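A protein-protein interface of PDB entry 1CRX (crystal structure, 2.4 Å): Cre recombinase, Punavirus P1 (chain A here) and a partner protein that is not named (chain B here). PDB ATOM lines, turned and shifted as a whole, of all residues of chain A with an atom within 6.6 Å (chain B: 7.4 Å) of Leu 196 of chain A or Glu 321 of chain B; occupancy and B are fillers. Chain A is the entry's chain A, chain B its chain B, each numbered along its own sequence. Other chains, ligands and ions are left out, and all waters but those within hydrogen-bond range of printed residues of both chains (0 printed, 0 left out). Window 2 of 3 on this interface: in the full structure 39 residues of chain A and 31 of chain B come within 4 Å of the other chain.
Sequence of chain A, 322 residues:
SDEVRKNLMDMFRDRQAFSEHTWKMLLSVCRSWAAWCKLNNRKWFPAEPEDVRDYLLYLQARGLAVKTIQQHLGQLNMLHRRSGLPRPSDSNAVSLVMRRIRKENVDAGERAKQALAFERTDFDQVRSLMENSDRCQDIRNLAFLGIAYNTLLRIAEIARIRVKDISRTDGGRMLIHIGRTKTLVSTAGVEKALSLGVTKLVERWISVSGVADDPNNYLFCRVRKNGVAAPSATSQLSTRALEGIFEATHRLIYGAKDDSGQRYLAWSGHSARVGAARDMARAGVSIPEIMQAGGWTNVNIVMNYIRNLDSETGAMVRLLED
Leu 196 of chain A touches just one residue of chain B: Glu 321 (2.8 Å). Glu 321 of chain B touches just these residues of chain A: Arg 173 (2.5 Å), Ser 195 (3.3 Å) and Leu 196 (2.8 Å). No residue of chain B comes within 4 Å of Gly 197 of chain A. Printed residues of chain A within 4 Å of Met 316 of chain B: Asn 150. Of the printed residues of chain B, Arg 120 of chain A touches Leu 319, Leu 320 and Asp 322. Of the printed residues of chain B, Asn 150 of chain A touches Met 316 and Leu 320. Of the printed residues of chain B, Leu 194 of chain A touches Val 317. Of the printed residues of chain A, Val 317 of chain B touches Arg 173 (3.7 Å), Leu 194 (3.9 Å) and Ser 195 (3.8 Å). Leu 201 of chain A touches none of the printed residues of chain B. Val 198 of chain A touches none of the printed residues of chain B. The nearest residue of chain B that does not touch Leu 196 of chain A is Val 317 of chain B (5.4 Å). The nearest printed residue of chain A that does not touch Asp 322 of chain B is Ser 195 of chain A (7.2 Å).
Of the 15 printed residues of chain A, 6 touch a printed residue of chain B. Hydrophobic or aromatic side chains of chain A that line the printed part of chain B: Leu 196. Printed residues of chain B that touch a printed residue of chain A: Met 316, Val 317, Leu 319, Leu 320, Glu 321 and Asp 322. Among the printed residues, Asp or Glu carboxylates within 4 Å of a Lys or Arg side-chain nitrogen of the other chain: Arg 173 of chain A with Glu 321 of chain B (2.5 Å).
The guanidinium group of Arg 120 of chain A lies within hydrogen-bond range of the backbone carbonyl oxygen of Leu 319 of chain B (2.7 Å). The backbone carbonyl oxygen (O) of Leu 320 of chain B lies within hydrogen-bond range of the guanidinium group (NH2) of Arg 120 of chain A (3.3 Å). The backbone carbonyl oxygen (O) of Asp 322 of chain B is in hydrogen-bond range of the guanidinium group (NH2) of Arg 120 of chain A. The guanidinium group of Arg 173 of chain A is in salt-bridge range of the side-chain carboxylate of Glu 321 of chain B (2.5 Å). OE2 of Glu 321 of chain B is in hydrogen-bond range of N of Leu 196 of chain A (2.8 Å).
The backbone NH (N) of Ser 195 of chain A lies within hydrogen-bond range of the side-chain amide oxygen (OD1) of Asn 150 of chain A, 3.1 Å away. The side-chain carboxylate of Asp 170 of chain A is in salt-bridge range of the guanidinium group of Arg 173 of chain A. The side-chain hydroxyl (OG1) of Thr 199 of chain A sits at hydrogen-bond distance from the backbone carbonyl oxygen (O) of Leu 194 of chain A, 3.3 Å away. N of Val 198 of chain A lies within hydrogen-bond range of OG of Ser 195 of chain A, 3.2 Å away. The backbone carbonyl oxygen (O) of Ser 195 of chain A lies within hydrogen-bond range of the side-chain hydroxyl (OG1) of Thr 199 of chain A (2.8 Å). The side-chain amino group (NZ) of Lys 200 of chain A lies close to the backbone carbonyl oxygen (O) of Leu 196 of chain A (3.4 Å).
Among the printed residues, merely in contact across the chains: Asn 150 of chain A with Met 316 of chain B (3.2 Å), Ser 195 of chain A with Glu 321 of chain B (3.3 Å), Asn 150 of chain A with Leu 320 of chain B (3.3 Å), Arg 173 of chain A with Val 317 of chain B (3.7 Å), Ser 195 of chain A with Val 317 of chain B (3.8 Å), Ser 195 of chain A with Leu 320 of chain B (3.8 Å) and Leu 194 of chain A with Val 317 of chain B (3.9 Å).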
ATOM      1  N   ARG A 120     -11.651  38.663   0.363  1.00  0.00           N
ATOM      2  CA  ARG A 120     -11.577  37.215   0.454  1.00  0.00           C
ATOM      3  C   ARG A 120     -10.269  36.833   1.124  1.00  0.00           C
ATOM      4  O   ARG A 120     -10.226  35.932   1.960  1.00  0.00           O
ATOM      5  CB  ARG A 120     -11.637  36.599  -0.947  1.00  0.00           C
ATOM      6  CG  ARG A 120     -11.161  35.155  -1.022  1.00  0.00           C
ATOM      7  CD  ARG A 120     -12.145  34.233  -0.323  1.00  0.00           C
ATOM      8  NE  ARG A 120     -11.884  32.833  -0.629  1.00  0.00           N
ATOM      9  CZ  ARG A 120     -12.548  32.132  -1.544  1.00  0.00           C
ATOM     10  NH1 ARG A 120     -13.520  32.699  -2.249  1.00  0.00           N
ATOM     11  NH2 ARG A 120     -12.240  30.861  -1.753  1.00  0.00           N
ATOM     12  N   ASN A 150     -20.379  37.384   2.352  1.00  0.00           N
ATOM     13  CA  ASN A 150     -21.082  36.560   1.384  1.00  0.00           C
ATOM     14  C   ASN A 150     -22.331  37.242   0.827  1.00  0.00           C
ATOM     15  O   ASN A 150     -22.578  37.202  -0.374  1.00  0.00           O
ATOM     16  CB  ASN A 150     -21.481  35.236   2.047  1.00  0.00           C
ATOM     17  CG  ASN A 150     -21.826  34.156   1.047  1.00  0.00           C
ATOM     18  OD1 ASN A 150     -21.896  32.974   1.395  1.00  0.00           O
ATOM     19  ND2 ASN A 150     -22.048  34.551  -0.201  1.00  0.00           N
ATOM     20  N   ASP A 170     -30.806  24.416  -2.482  1.00  0.00           N
ATOM     21  CA  ASP A 170     -30.108  23.276  -3.061  1.00  0.00           C
ATOM     22  C   ASP A 170     -28.693  23.053  -2.535  1.00  0.00           C
ATOM     23  O   ASP A 170     -27.945  23.998  -2.276  1.00  0.00           O
ATOM     24  CB  ASP A 170     -30.113  23.374  -4.598  1.00  0.00           C
ATOM     25  CG  ASP A 170     -29.060  24.322  -5.139  1.00  0.00           C
ATOM     26  OD1 ASP A 170     -27.854  24.023  -4.991  1.00  0.00           O
ATOM     27  OD2 ASP A 170     -29.445  25.362  -5.724  1.00  0.00           O
ATOM     28  N   GLY A 171     -28.344  21.782  -2.366  1.00  0.00           N
ATOM     29  CA  GLY A 171     -27.026  21.432  -1.877  1.00  0.00           C
ATOM     30  C   GLY A 171     -26.949  21.506  -0.371  1.00  0.00           C
ATOM     31  O   GLY A 171     -25.956  21.091   0.231  1.00  0.00           O
ATOM     32  N   GLY A 172     -28.003  22.037   0.239  1.00  0.00           N
ATOM     33  CA  GLY A 172     -28.030  22.161   1.684  1.00  0.00           C
ATOM     34  C   GLY A 172     -27.582  23.540   2.132  1.00  0.00           C
ATOM     35  O   GLY A 172     -27.654  23.879   3.319  1.00  0.00           O
ATOM     36  N   ARG A 173     -27.102  24.328   1.172  1.00  0.00           N
ATOM     37  CA  ARG A 173     -26.661  25.680   1.454  1.00  0.00           C
ATOM     38  C   ARG A 173     -27.822  26.382   2.134  1.00  0.00           C
ATOM     39  O   ARG A 173     -28.965  25.930   2.051  1.00  0.00           O
ATOM     40  CB  ARG A 173     -26.309  26.403   0.163  1.00  0.00           C
ATOM     41  CG  ARG A 173     -25.127  25.823  -0.556  1.00  0.00           C
ATOM     42  CD  ARG A 173     -24.722  26.736  -1.693  1.00  0.00           C
ATOM     43  NE  ARG A 173     -23.690  26.134  -2.530  1.00  0.00           N
ATOM     44  CZ  ARG A 173     -23.866  25.035  -3.258  1.00  0.00           C
ATOM     45  NH1 ARG A 173     -25.039  24.411  -3.254  1.00  0.00           N
ATOM     46  NH2 ARG A 173     -22.863  24.552  -3.983  1.00  0.00           N
ATOM     47  N   LEU A 194     -25.914  31.167   0.842  1.00  0.00           N
ATOM     48  CA  LEU A 194     -24.593  31.095   1.451  1.00  0.00           C
ATOM     49  C   LEU A 194     -23.842  29.876   0.922  1.00  0.00           C
ATOM     50  O   LEU A 194     -24.432  28.812   0.720  1.00  0.00           O
ATOM     51  CB  LEU A 194     -24.712  31.009   2.978  1.00  0.00           C
ATOM     52  CG  LEU A 194     -25.677  31.973   3.682  1.00  0.00           C
ATOM     53  CD1 LEU A 194     -25.585  31.745   5.185  1.00  0.00           C
ATOM     54  CD2 LEU A 194     -25.347  33.429   3.334  1.00  0.00           C
ATOM     55  N   SER A 195     -22.545  30.036   0.690  1.00  0.00           N
ATOM     56  CA  SER A 195     -21.736  28.937   0.196  1.00  0.00           C
ATOM     57  C   SER A 195     -21.839  27.765   1.163  1.00  0.00           C
ATOM     58  O   SER A 195     -22.474  27.863   2.213  1.00  0.00           O
ATOM     59  CB  SER A 195     -20.277  29.379   0.057  1.00  0.00           C
ATOM     60  OG  SER A 195     -19.667  29.523   1.322  1.00  0.00           O
ATOM     61  N   LEU A 196     -21.221  26.652   0.804  1.00  0.00           N
ATOM     62  CA  LEU A 196     -21.250  25.470   1.655  1.00  0.00           C
ATOM     63  C   LEU A 196     -20.502  25.744   2.955  1.00  0.00           C
ATOM     64  O   LEU A 196     -20.963  25.402   4.042  1.00  0.00           O
ATOM     65  CB  LEU A 196     -20.596  24.293   0.933  1.00  0.00           C
ATOM     66  CG  LEU A 196     -21.372  23.755  -0.269  1.00  0.00           C
ATOM     67  CD1 LEU A 196     -20.500  22.761  -1.011  1.00  0.00           C
ATOM     68  CD2 LEU A 196     -22.678  23.108   0.195  1.00  0.00           C
ATOM     69  N   GLY A 197     -19.340  26.365   2.817  1.00  0.00           N
ATOM     70  CA  GLY A 197     -18.516  26.694   3.955  1.00  0.00           C
ATOM     71  C   GLY A 197     -19.180  27.665   4.910  1.00  0.00           C
ATOM     72  O   GLY A 197     -19.334  27.368   6.095  1.00  0.00           O
ATOM     73  N   VAL A 198     -19.582  28.824   4.404  1.00  0.00           N
ATOM     74  CA  VAL A 198     -20.207  29.838   5.244  1.00  0.00           C
ATOM     75  C   VAL A 198     -21.464  29.309   5.931  1.00  0.00           C
ATOM     76  O   VAL A 198     -21.790  29.698   7.052  1.00  0.00           O
ATOM     77  CB  VAL A 198     -20.521  31.105   4.408  1.00  0.00           C
ATOM     78  CG1 VAL A 198     -21.297  32.127   5.232  1.00  0.00           C
ATOM     79  CG2 VAL A 198     -19.220  31.716   3.924  1.00  0.00           C
ATOM     80  N   THR A 199     -22.165  28.405   5.266  1.00  0.00           N
ATOM     81  CA  THR A 199     -23.371  27.836   5.843  1.00  0.00           C
ATOM     82  C   THR A 199     -22.957  26.964   7.019  1.00  0.00           C
ATOM     83  O   THR A 199     -23.666  26.858   8.020  1.00  0.00           O
ATOM     84  CB  THR A 199     -24.109  26.972   4.811  1.00  0.00           C
ATOM     85  OG1 THR A 199     -24.709  27.819   3.819  1.00  0.00           O
ATOM     86  CG2 THR A 199     -25.174  26.124   5.495  1.00  0.00           C
ATOM     87  N   LYS A 200     -21.797  26.332   6.881  1.00  0.00           N
ATOM     88  CA  LYS A 200     -21.268  25.475   7.927  1.00  0.00           C
ATOM     89  C   LYS A 200     -20.899  26.359   9.109  1.00  0.00           C
ATOM     90  O   LYS A 200     -21.201  26.023  10.252  1.00  0.00           O
ATOM     91  CB  LYS A 200     -20.030  24.724   7.429  1.00  0.00           C
ATOM     92  CG  LYS A 200     -20.332  23.557   6.493  1.00  0.00           C
ATOM     93  CD  LYS A 200     -19.054  22.830   6.049  1.00  0.00           C
ATOM     94  CE  LYS A 200     -18.445  23.442   4.780  1.00  0.00           C
ATOM     95  NZ  LYS A 200     -18.924  22.788   3.524  1.00  0.00           N
ATOM     96  N   LEU A 201     -20.249  27.488   8.829  1.00  0.00           N
ATOM     97  CA  LEU A 201     -19.852  28.434   9.871  1.00  0.00           C
ATOM     98  C   LEU A 201     -21.059  28.886  10.701  1.00  0.00           C
ATOM     99  O   LEU A 201     -21.008  28.907  11.933  1.00  0.00           O
ATOM    100  CB  LEU A 201     -19.194  29.662   9.249  1.00  0.00           C
ATOM    101  CG  LEU A 201     -17.763  29.543   8.737  1.00  0.00           C
ATOM    102  CD1 LEU A 201     -17.330  30.884   8.182  1.00  0.00           C
ATOM    103  CD2 LEU A 201     -16.834  29.125   9.850  1.00  0.00           C
ATOM    104  N   GLU A 203     -23.868  27.356  10.815  1.00  0.00           N
ATOM    105  CA  GLU A 203     -24.446  26.149  11.380  1.00  0.00           C
ATOM    106  C   GLU A 203     -23.878  25.918  12.774  1.00  0.00           C
ATOM    107  O   GLU A 203     -24.606  25.573  13.702  1.00  0.00           O
ATOM    108  CB  GLU A 203     -24.130  24.953  10.480  1.00  0.00           C
ATOM    109  CG  GLU A 203     -25.348  24.328   9.814  1.00  0.00           C
ATOM    110  CD  GLU A 203     -24.981  23.408   8.656  1.00  0.00           C
ATOM    111  OE1 GLU A 203     -23.773  23.281   8.336  1.00  0.00           O
ATOM    112  OE2 GLU A 203     -25.910  22.813   8.066  1.00  0.00           O
ATOM    113  N   MET B 316     -21.763  35.455  -5.430  1.00  0.00           N
ATOM    114  CA  MET B 316     -20.824  35.370  -4.323  1.00  0.00           C
ATOM    115  C   MET B 316     -20.594  33.924  -3.938  1.00  0.00           C
ATOM    116  O   MET B 316     -19.465  33.527  -3.673  1.00  0.00           O
ATOM    117  CB  MET B 316     -21.332  36.167  -3.121  1.00  0.00           C
ATOM    118  CG  MET B 316     -20.996  37.647  -3.179  1.00  0.00           C
ATOM    119  SD  MET B 316     -19.311  37.964  -3.712  1.00  0.00           S
ATOM    120  CE  MET B 316     -18.410  37.597  -2.228  1.00  0.00           C
ATOM    121  N   VAL B 317     -21.657  33.128  -3.922  1.00  0.00           N
ATOM    122  CA  VAL B 317     -21.520  31.719  -3.574  1.00  0.00           C
ATOM    123  C   VAL B 317     -20.469  31.060  -4.469  1.00  0.00           C
ATOM    124  O   VAL B 317     -19.561  30.392  -3.981  1.00  0.00           O
ATOM    125  CB  VAL B 317     -22.856  30.961  -3.726  1.00  0.00           C
ATOM    126  CG1 VAL B 317     -22.614  29.467  -3.633  1.00  0.00           C
ATOM    127  CG2 VAL B 317     -23.831  31.389  -2.639  1.00  0.00           C
ATOM    128  N   ARG B 318     -20.590  31.265  -5.779  1.00  0.00           N
ATOM    129  CA  ARG B 318     -19.649  30.694  -6.743  1.00  0.00           C
ATOM    130  C   ARG B 318     -18.235  31.185  -6.493  1.00  0.00           C
ATOM    131  O   ARG B 318     -17.270  30.471  -6.746  1.00  0.00           O
ATOM    132  CB  ARG B 318     -20.048  31.070  -8.171  1.00  0.00           C
ATOM    133  CG  ARG B 318     -21.139  30.198  -8.778  1.00  0.00           C
ATOM    134  CD  ARG B 318     -21.474  30.664 -10.189  1.00  0.00           C
ATOM    135  NE  ARG B 318     -22.700  31.460 -10.237  1.00  0.00           N
ATOM    136  CZ  ARG B 318     -22.772  32.711 -10.683  1.00  0.00           C
ATOM    137  NH1 ARG B 318     -21.686  33.340 -11.128  1.00  0.00           N
ATOM    138  NH2 ARG B 318     -23.943  33.331 -10.685  1.00  0.00           N
ATOM    139  N   LEU B 319     -18.121  32.413  -6.001  1.00  0.00           N
ATOM    140  CA  LEU B 319     -16.823  33.014  -5.723  1.00  0.00           C
ATOM    141  C   LEU B 319     -16.172  32.393  -4.490  1.00  0.00           C
ATOM    142  O   LEU B 319     -14.957  32.193  -4.444  1.00  0.00           O
ATOM    143  CB  LEU B 319     -16.986  34.519  -5.506  1.00  0.00           C
ATOM    144  CG  LEU B 319     -16.127  35.490  -6.317  1.00  0.00           C
ATOM    145  CD1 LEU B 319     -14.857  34.810  -6.802  1.00  0.00           C
ATOM    146  CD2 LEU B 319     -16.940  35.993  -7.489  1.00  0.00           C
ATOM    147  N   LEU B 320     -16.990  32.089  -3.490  1.00  0.00           N
ATOM    148  CA  LEU B 320     -16.488  31.507  -2.251  1.00  0.00           C
ATOM    149  C   LEU B 320     -16.191  30.023  -2.411  1.00  0.00           C
ATOM    150  O   LEU B 320     -15.233  29.506  -1.833  1.00  0.00           O
ATOM    151  CB  LEU B 320     -17.501  31.727  -1.116  1.00  0.00           C
ATOM    152  CG  LEU B 320     -17.327  33.047  -0.356  1.00  0.00           C
ATOM    153  CD1 LEU B 320     -18.678  33.622   0.037  1.00  0.00           C
ATOM    154  CD2 LEU B 320     -16.463  32.802   0.860  1.00  0.00           C
ATOM    155  N   GLU B 321     -17.006  29.341  -3.204  1.00  0.00           N
ATOM    156  CA  GLU B 321     -16.813  27.917  -3.416  1.00  0.00           C
ATOM    157  C   GLU B 321     -15.745  27.649  -4.476  1.00  0.00           C
ATOM    158  O   GLU B 321     -15.873  26.740  -5.292  1.00  0.00           O
ATOM    159  CB  GLU B 321     -18.152  27.266  -3.779  1.00  0.00           C
ATOM    160  CG  GLU B 321     -19.195  27.444  -2.670  1.00  0.00           C
ATOM    161  CD  GLU B 321     -20.488  26.684  -2.913  1.00  0.00           C
ATOM    162  OE1 GLU B 321     -20.736  26.271  -4.065  1.00  0.00           O
ATOM    163  OE2 GLU B 321     -21.260  26.504  -1.945  1.00  0.00           O
ATOM    164  N   ASP B 322     -14.686  28.455  -4.437  1.00  0.00           N
ATOM    165  CA  ASP B 322     -13.560  28.333  -5.355  1.00  0.00           C
ATOM    166  C   ASP B 322     -12.548  29.451  -5.130  1.00  0.00           C
ATOM    167  O   ASP B 322     -11.719  29.376  -4.221  1.00  0.00           O
ATOM    168  CB  ASP B 322     -14.037  28.365  -6.805  1.00  0.00           C
ATOM    169  CG  ASP B 322     -13.474  27.217  -7.624  1.00  0.00           C
ATOM    170  OD1 ASP B 322     -12.966  26.249  -7.010  1.00  0.00           O
ATOM    171  OD2 ASP B 322     -13.537  27.279  -8.873  1.00  0.00           O
